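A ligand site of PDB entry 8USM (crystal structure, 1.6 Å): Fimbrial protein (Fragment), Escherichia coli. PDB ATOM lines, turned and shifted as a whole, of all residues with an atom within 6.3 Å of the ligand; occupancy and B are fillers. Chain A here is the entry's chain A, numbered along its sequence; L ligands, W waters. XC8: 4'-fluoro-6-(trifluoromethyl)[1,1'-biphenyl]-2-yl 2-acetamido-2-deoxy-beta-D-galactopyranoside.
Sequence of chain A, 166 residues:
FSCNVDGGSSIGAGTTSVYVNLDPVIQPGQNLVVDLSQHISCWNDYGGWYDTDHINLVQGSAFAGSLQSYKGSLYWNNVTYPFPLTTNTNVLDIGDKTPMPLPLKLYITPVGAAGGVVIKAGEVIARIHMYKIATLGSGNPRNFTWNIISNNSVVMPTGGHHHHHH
O09 of the ligand sits at hydrogen-bond distance from OD1 of Asp 53 (2.6 Å).
An oxygen (O12) of the ligand is in hydrogen-bond range of the backbone NH of Phe 1.
The side-chain amino group of Lys 132 is in hydrogen-bond range of an oxygen (O09) of the ligand (2.9 Å).
An oxygen (O12) of the ligand sits at hydrogen-bond distance from the backbone NH of Asp 45, 2.9 Å away.
The guanidinium group of Arg 142 sits at hydrogen-bond distance from an oxygen (O03) of the ligand, 2.9 Å away.
An oxygen (O07) of the ligand lies within hydrogen-bond range of the side-chain amide nitrogen of Asn 140 (3.3 Å).
The side-chain amide nitrogen of Asn 44 sits at hydrogen-bond distance from the side-chain carboxylate of Asp 53 (3.1 Å).
NZ of Lys 132 lies within hydrogen-bond range of O of Asn 140, at 2.8 Å.
The side-chain amino group (NZ) of Lys 132 lies within hydrogen-bond range of the backbone carbonyl oxygen (O) of Gly 139.
OD2 of Asp 45 lies within hydrogen-bond range of OG of Ser 2 (2.7 Å).
The side-chain carboxylate of Asp 45 lies within hydrogen-bond range of the indole nitrogen of Trp 43 (3.2 Å).
OD1 of Asp 51 lies within hydrogen-bond range of N of Leu 136, 2.9 Å away.
N of Ala 134 sits at hydrogen-bond distance from O of Gly 139 (2.8 Å).
The side-chain hydroxyl (OG) of Ser 2 lies close to the side-chain hydroxyl (OG) of Ser 10 (3.2 Å).
Merely in contact with the ligand: Asn 44 (3.3 Å), Asp 51 (3.4 Å), Ala 134 (3.4 Å), Tyr 46 (3.4 Å), Gly 12 (3.5 Å), Gly 139 (3.5 Å) and Ser 2 (3.8 Å).
Hydrophobic or aromatic side chains that line the ligand: Phe 1, Tyr 46 and Ala 134.
The nearest printed residue that does not touch the ligand is Trp 43 (4.5 Å).
Water W3 lies within hydrogen-bond range of an oxygen (O03) of the ligand (2.7 Å), the side-chain amino group of Lys 132 (2.8 Å) and the backbone NH of Phe 1 (3.1 Å).
Water W2 lies within hydrogen-bond range of the side-chain carboxylate of Asp 51 (2.6 Å), an oxygen (O07) of the ligand (2.8 Å), the backbone carbonyl oxygen of Leu 136 (2.9 Å) and the side-chain amide nitrogen of Asn 140 (3.2 Å).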
ATOM      1  N   PHE A   1     -25.666 -11.731  -9.892  1.00  0.00           N
ATOM      2  CA  PHE A   1     -26.152 -12.414 -11.126  1.00  0.00           C
ATOM      3  C   PHE A   1     -25.718 -11.663 -12.372  1.00  0.00           C
ATOM      4  O   PHE A   1     -25.880 -10.446 -12.459  1.00  0.00           O
ATOM      5  CB  PHE A   1     -27.670 -12.548 -11.092  1.00  0.00           C
ATOM      6  CG  PHE A   1     -28.242 -13.162 -12.326  1.00  0.00           C
ATOM      7  CD1 PHE A   1     -28.802 -12.379 -13.325  1.00  0.00           C
ATOM      8  CD2 PHE A   1     -28.241 -14.538 -12.493  1.00  0.00           C
ATOM      9  CE1 PHE A   1     -29.338 -12.950 -14.451  1.00  0.00           C
ATOM     10  CE2 PHE A   1     -28.777 -15.109 -13.619  1.00  0.00           C
ATOM     11  CZ  PHE A   1     -29.325 -14.313 -14.605  1.00  0.00           C
ATOM     12  N   SER A   2     -25.182 -12.383 -13.351  1.00  0.00           N
ATOM     13  CA  SER A   2     -24.680 -11.766 -14.568  1.00  0.00           C
ATOM     14  C   SER A   2     -24.933 -12.688 -15.750  1.00  0.00           C
ATOM     15  O   SER A   2     -25.095 -13.897 -15.598  1.00  0.00           O
ATOM     16  CB  SER A   2     -23.189 -11.430 -14.455  1.00  0.00           C
ATOM     17  OG  SER A   2     -22.934 -10.506 -13.422  1.00  0.00           O
ATOM     18  N   SER A  10     -19.579  -9.080 -19.157  1.00  0.00           N
ATOM     19  CA  SER A  10     -20.651  -9.373 -18.210  1.00  0.00           C
ATOM     20  C   SER A  10     -21.722  -8.303 -18.252  1.00  0.00           C
ATOM     21  O   SER A  10     -21.432  -7.105 -18.419  1.00  0.00           O
ATOM     22  CB  SER A  10     -20.047  -9.494 -16.808  1.00  0.00           C
ATOM     23  OG  SER A  10     -21.030  -9.791 -15.839  1.00  0.00           O
ATOM     24  N   ILE A  11     -22.965  -8.735 -18.106  1.00  0.00           N
ATOM     25  CA  ILE A  11     -24.143  -7.875 -18.146  1.00  0.00           C
ATOM     26  C   ILE A  11     -24.905  -8.068 -16.840  1.00  0.00           C
ATOM     27  O   ILE A  11     -25.252  -9.197 -16.490  1.00  0.00           O
ATOM     28  CB  ILE A  11     -25.050  -8.221 -19.341  1.00  0.00           C
ATOM     29  CG1 ILE A  11     -24.271  -8.174 -20.649  1.00  0.00           C
ATOM     30  CG2 ILE A  11     -26.243  -7.283 -19.378  1.00  0.00           C
ATOM     31  CD1 ILE A  11     -24.982  -8.861 -21.777  1.00  0.00           C
ATOM     32  N   GLY A  12     -25.202  -6.963 -16.160  1.00  0.00           N
ATOM     33  CA  GLY A  12     -25.910  -7.041 -14.894  1.00  0.00           C
ATOM     34  C   GLY A  12     -27.377  -6.647 -14.971  1.00  0.00           C
ATOM     35  O   GLY A  12     -28.155  -6.925 -14.061  1.00  0.00           O
ATOM     36  N   ALA A  13     -27.743  -5.989 -16.054  1.00  0.00           N
ATOM     37  CA  ALA A  13     -29.099  -5.490 -16.236  1.00  0.00           C
ATOM     38  C   ALA A  13     -29.129  -4.797 -17.586  1.00  0.00           C
ATOM     39  O   ALA A  13     -28.090  -4.552 -18.207  1.00  0.00           O
ATOM     40  CB  ALA A  13     -29.504  -4.503 -15.142  1.00  0.00           C
ATOM     41  N   TRP A  43     -24.996 -16.632 -15.035  1.00  0.00           N
ATOM     42  CA  TRP A  43     -24.377 -17.327 -13.920  1.00  0.00           C
ATOM     43  C   TRP A  43     -24.629 -16.567 -12.619  1.00  0.00           C
ATOM     44  O   TRP A  43     -25.063 -15.418 -12.602  1.00  0.00           O
ATOM     45  CB  TRP A  43     -22.868 -17.502 -14.140  1.00  0.00           C
ATOM     46  CG  TRP A  43     -22.183 -16.209 -14.323  1.00  0.00           C
ATOM     47  CD1 TRP A  43     -21.612 -15.438 -13.359  1.00  0.00           C
ATOM     48  CD2 TRP A  43     -22.003 -15.514 -15.557  1.00  0.00           C
ATOM     49  NE1 TRP A  43     -21.091 -14.298 -13.922  1.00  0.00           N
ATOM     50  CE2 TRP A  43     -21.306 -14.326 -15.266  1.00  0.00           C
ATOM     51  CE3 TRP A  43     -22.364 -15.773 -16.886  1.00  0.00           C
ATOM     52  CZ2 TRP A  43     -20.974 -13.399 -16.244  1.00  0.00           C
ATOM     53  CZ3 TRP A  43     -22.021 -14.866 -17.863  1.00  0.00           C
ATOM     54  CH2 TRP A  43     -21.327 -13.691 -17.531  1.00  0.00           C
ATOM     55  N   ASN A  44     -24.357 -17.284 -11.533  1.00  0.00           N
ATOM     56  CA  ASN A  44     -24.404 -16.748 -10.185  1.00  0.00           C
ATOM     57  C   ASN A  44     -23.040 -16.162  -9.842  1.00  0.00           C
ATOM     58  O   ASN A  44     -22.014 -16.813 -10.061  1.00  0.00           O
ATOM     59  CB  ASN A  44     -24.783 -17.869  -9.222  1.00  0.00           C
ATOM     60  CG  ASN A  44     -24.991 -17.391  -7.832  1.00  0.00           C
ATOM     61  OD1 ASN A  44     -24.034 -17.014  -7.168  1.00  0.00           O
ATOM     62  ND2 ASN A  44     -26.236 -17.403  -7.375  1.00  0.00           N
ATOM     63  N   ASP A  45     -23.024 -14.937  -9.335  1.00  0.00           N
ATOM     64  CA  ASP A  45     -21.738 -14.264  -9.172  1.00  0.00           C
ATOM     65  C   ASP A  45     -20.976 -14.678  -7.929  1.00  0.00           C
ATOM     66  O   ASP A  45     -19.812 -14.299  -7.785  1.00  0.00           O
ATOM     67  CB  ASP A  45     -21.948 -12.741  -9.184  1.00  0.00           C
ATOM     68  CG  ASP A  45     -22.053 -12.205 -10.585  1.00  0.00           C
ATOM     69  OD1 ASP A  45     -21.095 -12.421 -11.367  1.00  0.00           O
ATOM     70  OD2 ASP A  45     -23.091 -11.617 -10.919  1.00  0.00           O
ATOM     71  N   TYR A  46     -21.577 -15.474  -7.042  1.00  0.00           N
ATOM     72  CA  TYR A  46     -20.870 -16.056  -5.911  1.00  0.00           C
ATOM     73  C   TYR A  46     -20.565 -17.525  -6.105  1.00  0.00           C
ATOM     74  O   TYR A  46     -19.517 -18.007  -5.652  1.00  0.00           O
ATOM     75  CB  TYR A  46     -21.696 -15.890  -4.633  1.00  0.00           C
ATOM     76  CG  TYR A  46     -21.931 -14.457  -4.228  1.00  0.00           C
ATOM     77  CD1 TYR A  46     -23.187 -14.033  -3.836  1.00  0.00           C
ATOM     78  CD2 TYR A  46     -20.895 -13.545  -4.224  1.00  0.00           C
ATOM     79  CE1 TYR A  46     -23.408 -12.729  -3.450  1.00  0.00           C
ATOM     80  CE2 TYR A  46     -21.103 -12.239  -3.844  1.00  0.00           C
ATOM     81  CZ  TYR A  46     -22.359 -11.831  -3.457  1.00  0.00           C
ATOM     82  OH  TYR A  46     -22.576 -10.535  -3.081  1.00  0.00           O
ATOM     83  N   GLY A  47     -21.449 -18.258  -6.769  1.00  0.00           N
ATOM     84  CA  GLY A  47     -21.315 -19.687  -6.883  1.00  0.00           C
ATOM     85  C   GLY A  47     -21.739 -20.383  -5.603  1.00  0.00           C
ATOM     86  O   GLY A  47     -22.131 -19.776  -4.612  1.00  0.00           O
ATOM     87  N   ASP A  51     -26.406 -17.546  -2.673  1.00  0.00           N
ATOM     88  CA  ASP A  51     -27.510 -16.605  -2.873  1.00  0.00           C
ATOM     89  C   ASP A  51     -28.099 -16.890  -4.246  1.00  0.00           C
ATOM     90  O   ASP A  51     -27.770 -16.235  -5.233  1.00  0.00           O
ATOM     91  CB  ASP A  51     -27.012 -15.155  -2.759  1.00  0.00           C
ATOM     92  CG  ASP A  51     -28.125 -14.127  -2.871  1.00  0.00           C
ATOM     93  OD1 ASP A  51     -29.316 -14.497  -2.917  1.00  0.00           O
ATOM     94  OD2 ASP A  51     -27.790 -12.928  -2.921  1.00  0.00           O
ATOM     95  N   THR A  52     -28.968 -17.901  -4.321  1.00  0.00           N
ATOM     96  CA  THR A  52     -29.402 -18.439  -5.592  1.00  0.00           C
ATOM     97  C   THR A  52     -30.239 -17.419  -6.363  1.00  0.00           C
ATOM     98  O   THR A  52     -31.085 -16.721  -5.792  1.00  0.00           O
ATOM     99  CB  THR A  52     -30.200 -19.720  -5.377  1.00  0.00           C
ATOM    100  OG1 THR A  52     -29.366 -20.720  -4.794  1.00  0.00           O
ATOM    101  CG2 THR A  52     -30.775 -20.255  -6.682  1.00  0.00           C
ATOM    102  N   ASP A  53     -29.983 -17.333  -7.659  1.00  0.00           N
ATOM    103  CA  ASP A  53     -30.735 -16.462  -8.540  1.00  0.00           C
ATOM    104  C   ASP A  53     -31.916 -17.183  -9.151  1.00  0.00           C
ATOM    105  O   ASP A  53     -31.850 -18.376  -9.453  1.00  0.00           O
ATOM    106  CB  ASP A  53     -29.823 -15.930  -9.638  1.00  0.00           C
ATOM    107  CG  ASP A  53     -28.710 -15.086  -9.074  1.00  0.00           C
ATOM    108  OD1 ASP A  53     -29.042 -14.122  -8.355  1.00  0.00           O
ATOM    109  OD2 ASP A  53     -27.522 -15.379  -9.324  1.00  0.00           O
ATOM    110  N   ILE A  94     -30.413 -20.398 -10.751  1.00  0.00           N
ATOM    111  CA  ILE A  94     -29.019 -20.351 -11.147  1.00  0.00           C
ATOM    112  C   ILE A  94     -28.173 -20.081  -9.900  1.00  0.00           C
ATOM    113  O   ILE A  94     -28.327 -19.028  -9.263  1.00  0.00           O
ATOM    114  CB  ILE A  94     -28.775 -19.283 -12.228  1.00  0.00           C
ATOM    115  CG1 ILE A  94     -29.437 -19.752 -13.518  1.00  0.00           C
ATOM    116  CG2 ILE A  94     -27.296 -18.999 -12.410  1.00  0.00           C
ATOM    117  CD1 ILE A  94     -29.293 -18.800 -14.677  1.00  0.00           C
ATOM    118  N   LYS A 132     -34.879 -11.086 -12.960  1.00  0.00           N
ATOM    119  CA  LYS A 132     -34.036 -11.784 -12.006  1.00  0.00           C
ATOM    120  C   LYS A 132     -34.356 -11.290 -10.597  1.00  0.00           C
ATOM    121  O   LYS A 132     -34.482 -10.093 -10.374  1.00  0.00           O
ATOM    122  CB  LYS A 132     -32.549 -11.565 -12.306  1.00  0.00           C
ATOM    123  CG  LYS A 132     -31.620 -12.001 -11.182  1.00  0.00           C
ATOM    124  CD  LYS A 132     -31.211 -10.826 -10.277  1.00  0.00           C
ATOM    125  CE  LYS A 132     -30.496 -11.295  -8.996  1.00  0.00           C
ATOM    126  NZ  LYS A 132     -29.815 -10.171  -8.278  1.00  0.00           N
ATOM    127  N   ILE A 133     -34.451 -12.227  -9.669  1.00  0.00           N
ATOM    128  CA  ILE A 133     -34.483 -11.907  -8.241  1.00  0.00           C
ATOM    129  C   ILE A 133     -33.772 -13.047  -7.536  1.00  0.00           C
ATOM    130  O   ILE A 133     -33.939 -14.218  -7.896  1.00  0.00           O
ATOM    131  CB  ILE A 133     -35.922 -11.684  -7.737  1.00  0.00           C
ATOM    132  CG1 ILE A 133     -35.873 -11.068  -6.331  1.00  0.00           C
ATOM    133  CG2 ILE A 133     -36.740 -12.944  -7.749  1.00  0.00           C
ATOM    134  CD1 ILE A 133     -37.217 -10.548  -5.832  1.00  0.00           C
ATOM    135  N   ALA A 134     -32.924 -12.712  -6.573  1.00  0.00           N
ATOM    136  CA  ALA A 134     -32.114 -13.703  -5.869  1.00  0.00           C
ATOM    137  C   ALA A 134     -32.834 -14.134  -4.602  1.00  0.00           C
ATOM    138  O   ALA A 134     -34.066 -14.096  -4.530  1.00  0.00           O
ATOM    139  CB  ALA A 134     -30.712 -13.153  -5.588  1.00  0.00           C
ATOM    140  N   THR A 135     -32.077 -14.539  -3.587  1.00  0.00           N
ATOM    141  CA  THR A 135     -32.660 -15.203  -2.423  1.00  0.00           C
ATOM    142  C   THR A 135     -32.483 -14.422  -1.138  1.00  0.00           C
ATOM    143  O   THR A 135     -33.429 -14.327  -0.342  1.00  0.00           O
ATOM    144  CB  THR A 135     -32.034 -16.603  -2.275  1.00  0.00           C
ATOM    145  OG1 THR A 135     -32.278 -17.376  -3.466  1.00  0.00           O
ATOM    146  CG2 THR A 135     -32.600 -17.352  -1.077  1.00  0.00           C
ATOM    147  N   LEU A 136     -31.308 -13.838  -0.932  1.00  0.00           N
ATOM    148  CA  LEU A 136     -30.965 -13.144   0.301  1.00  0.00           C
ATOM    149  C   LEU A 136     -31.438 -11.693   0.243  1.00  0.00           C
ATOM    150  O   LEU A 136     -31.454 -11.061  -0.819  1.00  0.00           O
ATOM    151  CB  LEU A 136     -29.454 -13.194   0.527  1.00  0.00           C
ATOM    152  CG  LEU A 136     -28.838 -14.587   0.654  1.00  0.00           C
ATOM    153  CD1 LEU A 136     -27.334 -14.504   0.848  1.00  0.00           C
ATOM    154  CD2 LEU A 136     -29.491 -15.355   1.792  1.00  0.00           C
ATOM    155  N   GLY A 139     -33.232  -9.699  -2.597  1.00  0.00           N
ATOM    156  CA  GLY A 139     -32.991 -10.383  -3.851  1.00  0.00           C
ATOM    157  C   GLY A 139     -32.448  -9.515  -4.966  1.00  0.00           C
ATOM    158  O   GLY A 139     -32.153 -10.047  -6.045  1.00  0.00           O
ATOM    159  N   ASN A 140     -32.310  -8.203  -4.733  1.00  0.00           N
ATOM    160  CA  ASN A 140     -31.741  -7.251  -5.683  1.00  0.00           C
ATOM    161  C   ASN A 140     -32.253  -7.511  -7.085  1.00  0.00           C
ATOM    162  O   ASN A 140     -31.480  -7.881  -7.987  1.00  0.00           O
ATOM    163  CB  ASN A 140     -30.212  -7.340  -5.634  1.00  0.00           C
ATOM    164  CG  ASN A 140     -29.659  -6.912  -4.284  1.00  0.00           C
ATOM    165  OD1 ASN A 140     -29.816  -5.761  -3.884  1.00  0.00           O
ATOM    166  ND2 ASN A 140     -29.005  -7.842  -3.581  1.00  0.00           N
ATOM    167  N   PRO A 141     -33.537  -7.295  -7.303  1.00  0.00           N
ATOM    168  CA  PRO A 141     -34.134  -7.640  -8.606  1.00  0.00           C
ATOM    169  C   PRO A 141     -33.567  -6.802  -9.744  1.00  0.00           C
ATOM    170  O   PRO A 141     -33.199  -5.639  -9.579  1.00  0.00           O
ATOM    171  CB  PRO A 141     -35.627  -7.355  -8.408  1.00  0.00           C
ATOM    172  CG  PRO A 141     -35.696  -6.449  -7.199  1.00  0.00           C
ATOM    173  CD  PRO A 141     -34.562  -6.891  -6.330  1.00  0.00           C
ATOM    174  N   ARG A 142     -33.510  -7.431 -10.906  1.00  0.00           N
ATOM    175  CA  ARG A 142     -32.960  -6.809 -12.087  1.00  0.00           C
ATOM    176  C   ARG A 142     -33.810  -7.160 -13.294  1.00  0.00           C
ATOM    177  O   ARG A 142     -34.379  -8.254 -13.386  1.00  0.00           O
ATOM    178  CB  ARG A 142     -31.537  -7.267 -12.379  1.00  0.00           C
ATOM    179  CG  ARG A 142     -30.633  -7.171 -11.222  1.00  0.00           C
ATOM    180  CD  ARG A 142     -30.214  -5.750 -10.997  1.00  0.00           C
ATOM    181  NE  ARG A 142     -29.298  -5.696  -9.876  1.00  0.00           N
ATOM    182  CZ  ARG A 142     -28.490  -4.675  -9.608  1.00  0.00           C
ATOM    183  NH1 ARG A 142     -28.474  -3.621 -10.407  1.00  0.00           N
ATOM    184  NH2 ARG A 142     -27.695  -4.734  -8.557  1.00  0.00           N
HETATM  185  C11 XC8 L   1     -25.609 -14.081  -6.954  1.00  0.00           C
HETATM  186  C10 XC8 L   1     -25.803 -12.746  -6.316  1.00  0.00           C
HETATM  187  C01 XC8 L   1     -26.749  -6.079  -5.708  1.00  0.00           C
HETATM  188  C02 XC8 L   1     -26.823  -7.428  -6.456  1.00  0.00           C
HETATM  189  C05 XC8 L   1     -26.448  -9.953  -6.398  1.00  0.00           C
HETATM  190  C06 XC8 L   1     -27.296 -10.918  -5.633  1.00  0.00           C
HETATM  191  C08 XC8 L   1     -27.216 -12.241  -6.329  1.00  0.00           C
HETATM  192  C14 XC8 L   1     -24.986 -10.426  -6.542  1.00  0.00           C
HETATM  193  C16 XC8 L   1     -22.984  -9.614  -7.408  1.00  0.00           C
HETATM  194  C17 XC8 L   1     -22.219 -10.419  -6.601  1.00  0.00           C
HETATM  195  C18 XC8 L   1     -20.795 -10.389  -6.730  1.00  0.00           C
HETATM  196  C19 XC8 L   1     -20.185  -9.518  -7.681  1.00  0.00           C
HETATM  197  C20 XC8 L   1     -20.970  -8.721  -8.500  1.00  0.00           C
HETATM  198  C21 XC8 L   1     -20.338  -7.784  -9.540  1.00  0.00           C
HETATM  199  C25 XC8 L   1     -22.370  -8.752  -8.369  1.00  0.00           C
HETATM  200  C26 XC8 L   1     -23.363  -7.907  -9.220  1.00  0.00           C
HETATM  201  C27 XC8 L   1     -23.811  -8.410 -10.428  1.00  0.00           C
HETATM  202  C28 XC8 L   1     -24.738  -7.680 -11.199  1.00  0.00           C
HETATM  203  C29 XC8 L   1     -25.207  -6.457 -10.727  1.00  0.00           C
HETATM  204  C31 XC8 L   1     -24.768  -5.939  -9.485  1.00  0.00           C
HETATM  205  C32 XC8 L   1     -23.853  -6.667  -8.722  1.00  0.00           C
HETATM  206  F22 XC8 L   1     -20.721  -8.121 -10.799  1.00  0.00           F
HETATM  207  F23 XC8 L   1     -18.962  -7.887  -9.433  1.00  0.00           F
HETATM  208  F24 XC8 L   1     -20.721  -6.489  -9.253  1.00  0.00           F
HETATM  209  F30 XC8 L   1     -26.108  -5.749 -11.466  1.00  0.00           F
HETATM  210  N04 XC8 L   1     -26.400  -8.637  -5.731  1.00  0.00           N
HETATM  211  O03 XC8 L   1     -27.233  -7.474  -7.598  1.00  0.00           O
HETATM  212  O07 XC8 L   1     -28.649 -10.418  -5.636  1.00  0.00           O
HETATM  213  O09 XC8 L   1     -27.710 -12.038  -7.658  1.00  0.00           O
HETATM  214  O12 XC8 L   1     -25.590 -13.938  -8.340  1.00  0.00           O
HETATM  215  O13 XC8 L   1     -24.897 -11.774  -7.074  1.00  0.00           O
HETATM  216  O15 XC8 L   1     -24.383  -9.553  -7.388  1.00  0.00           O
HETATM  217  O   HOH W   1     -25.723  -9.001  -2.855  1.00  0.00           O
HETATM  218  O   HOH W   2     -29.545 -10.966  -3.061  1.00  0.00           O
HETATM  219  O   HOH W   3     -27.559  -9.246  -9.653  1.00  0.00           O
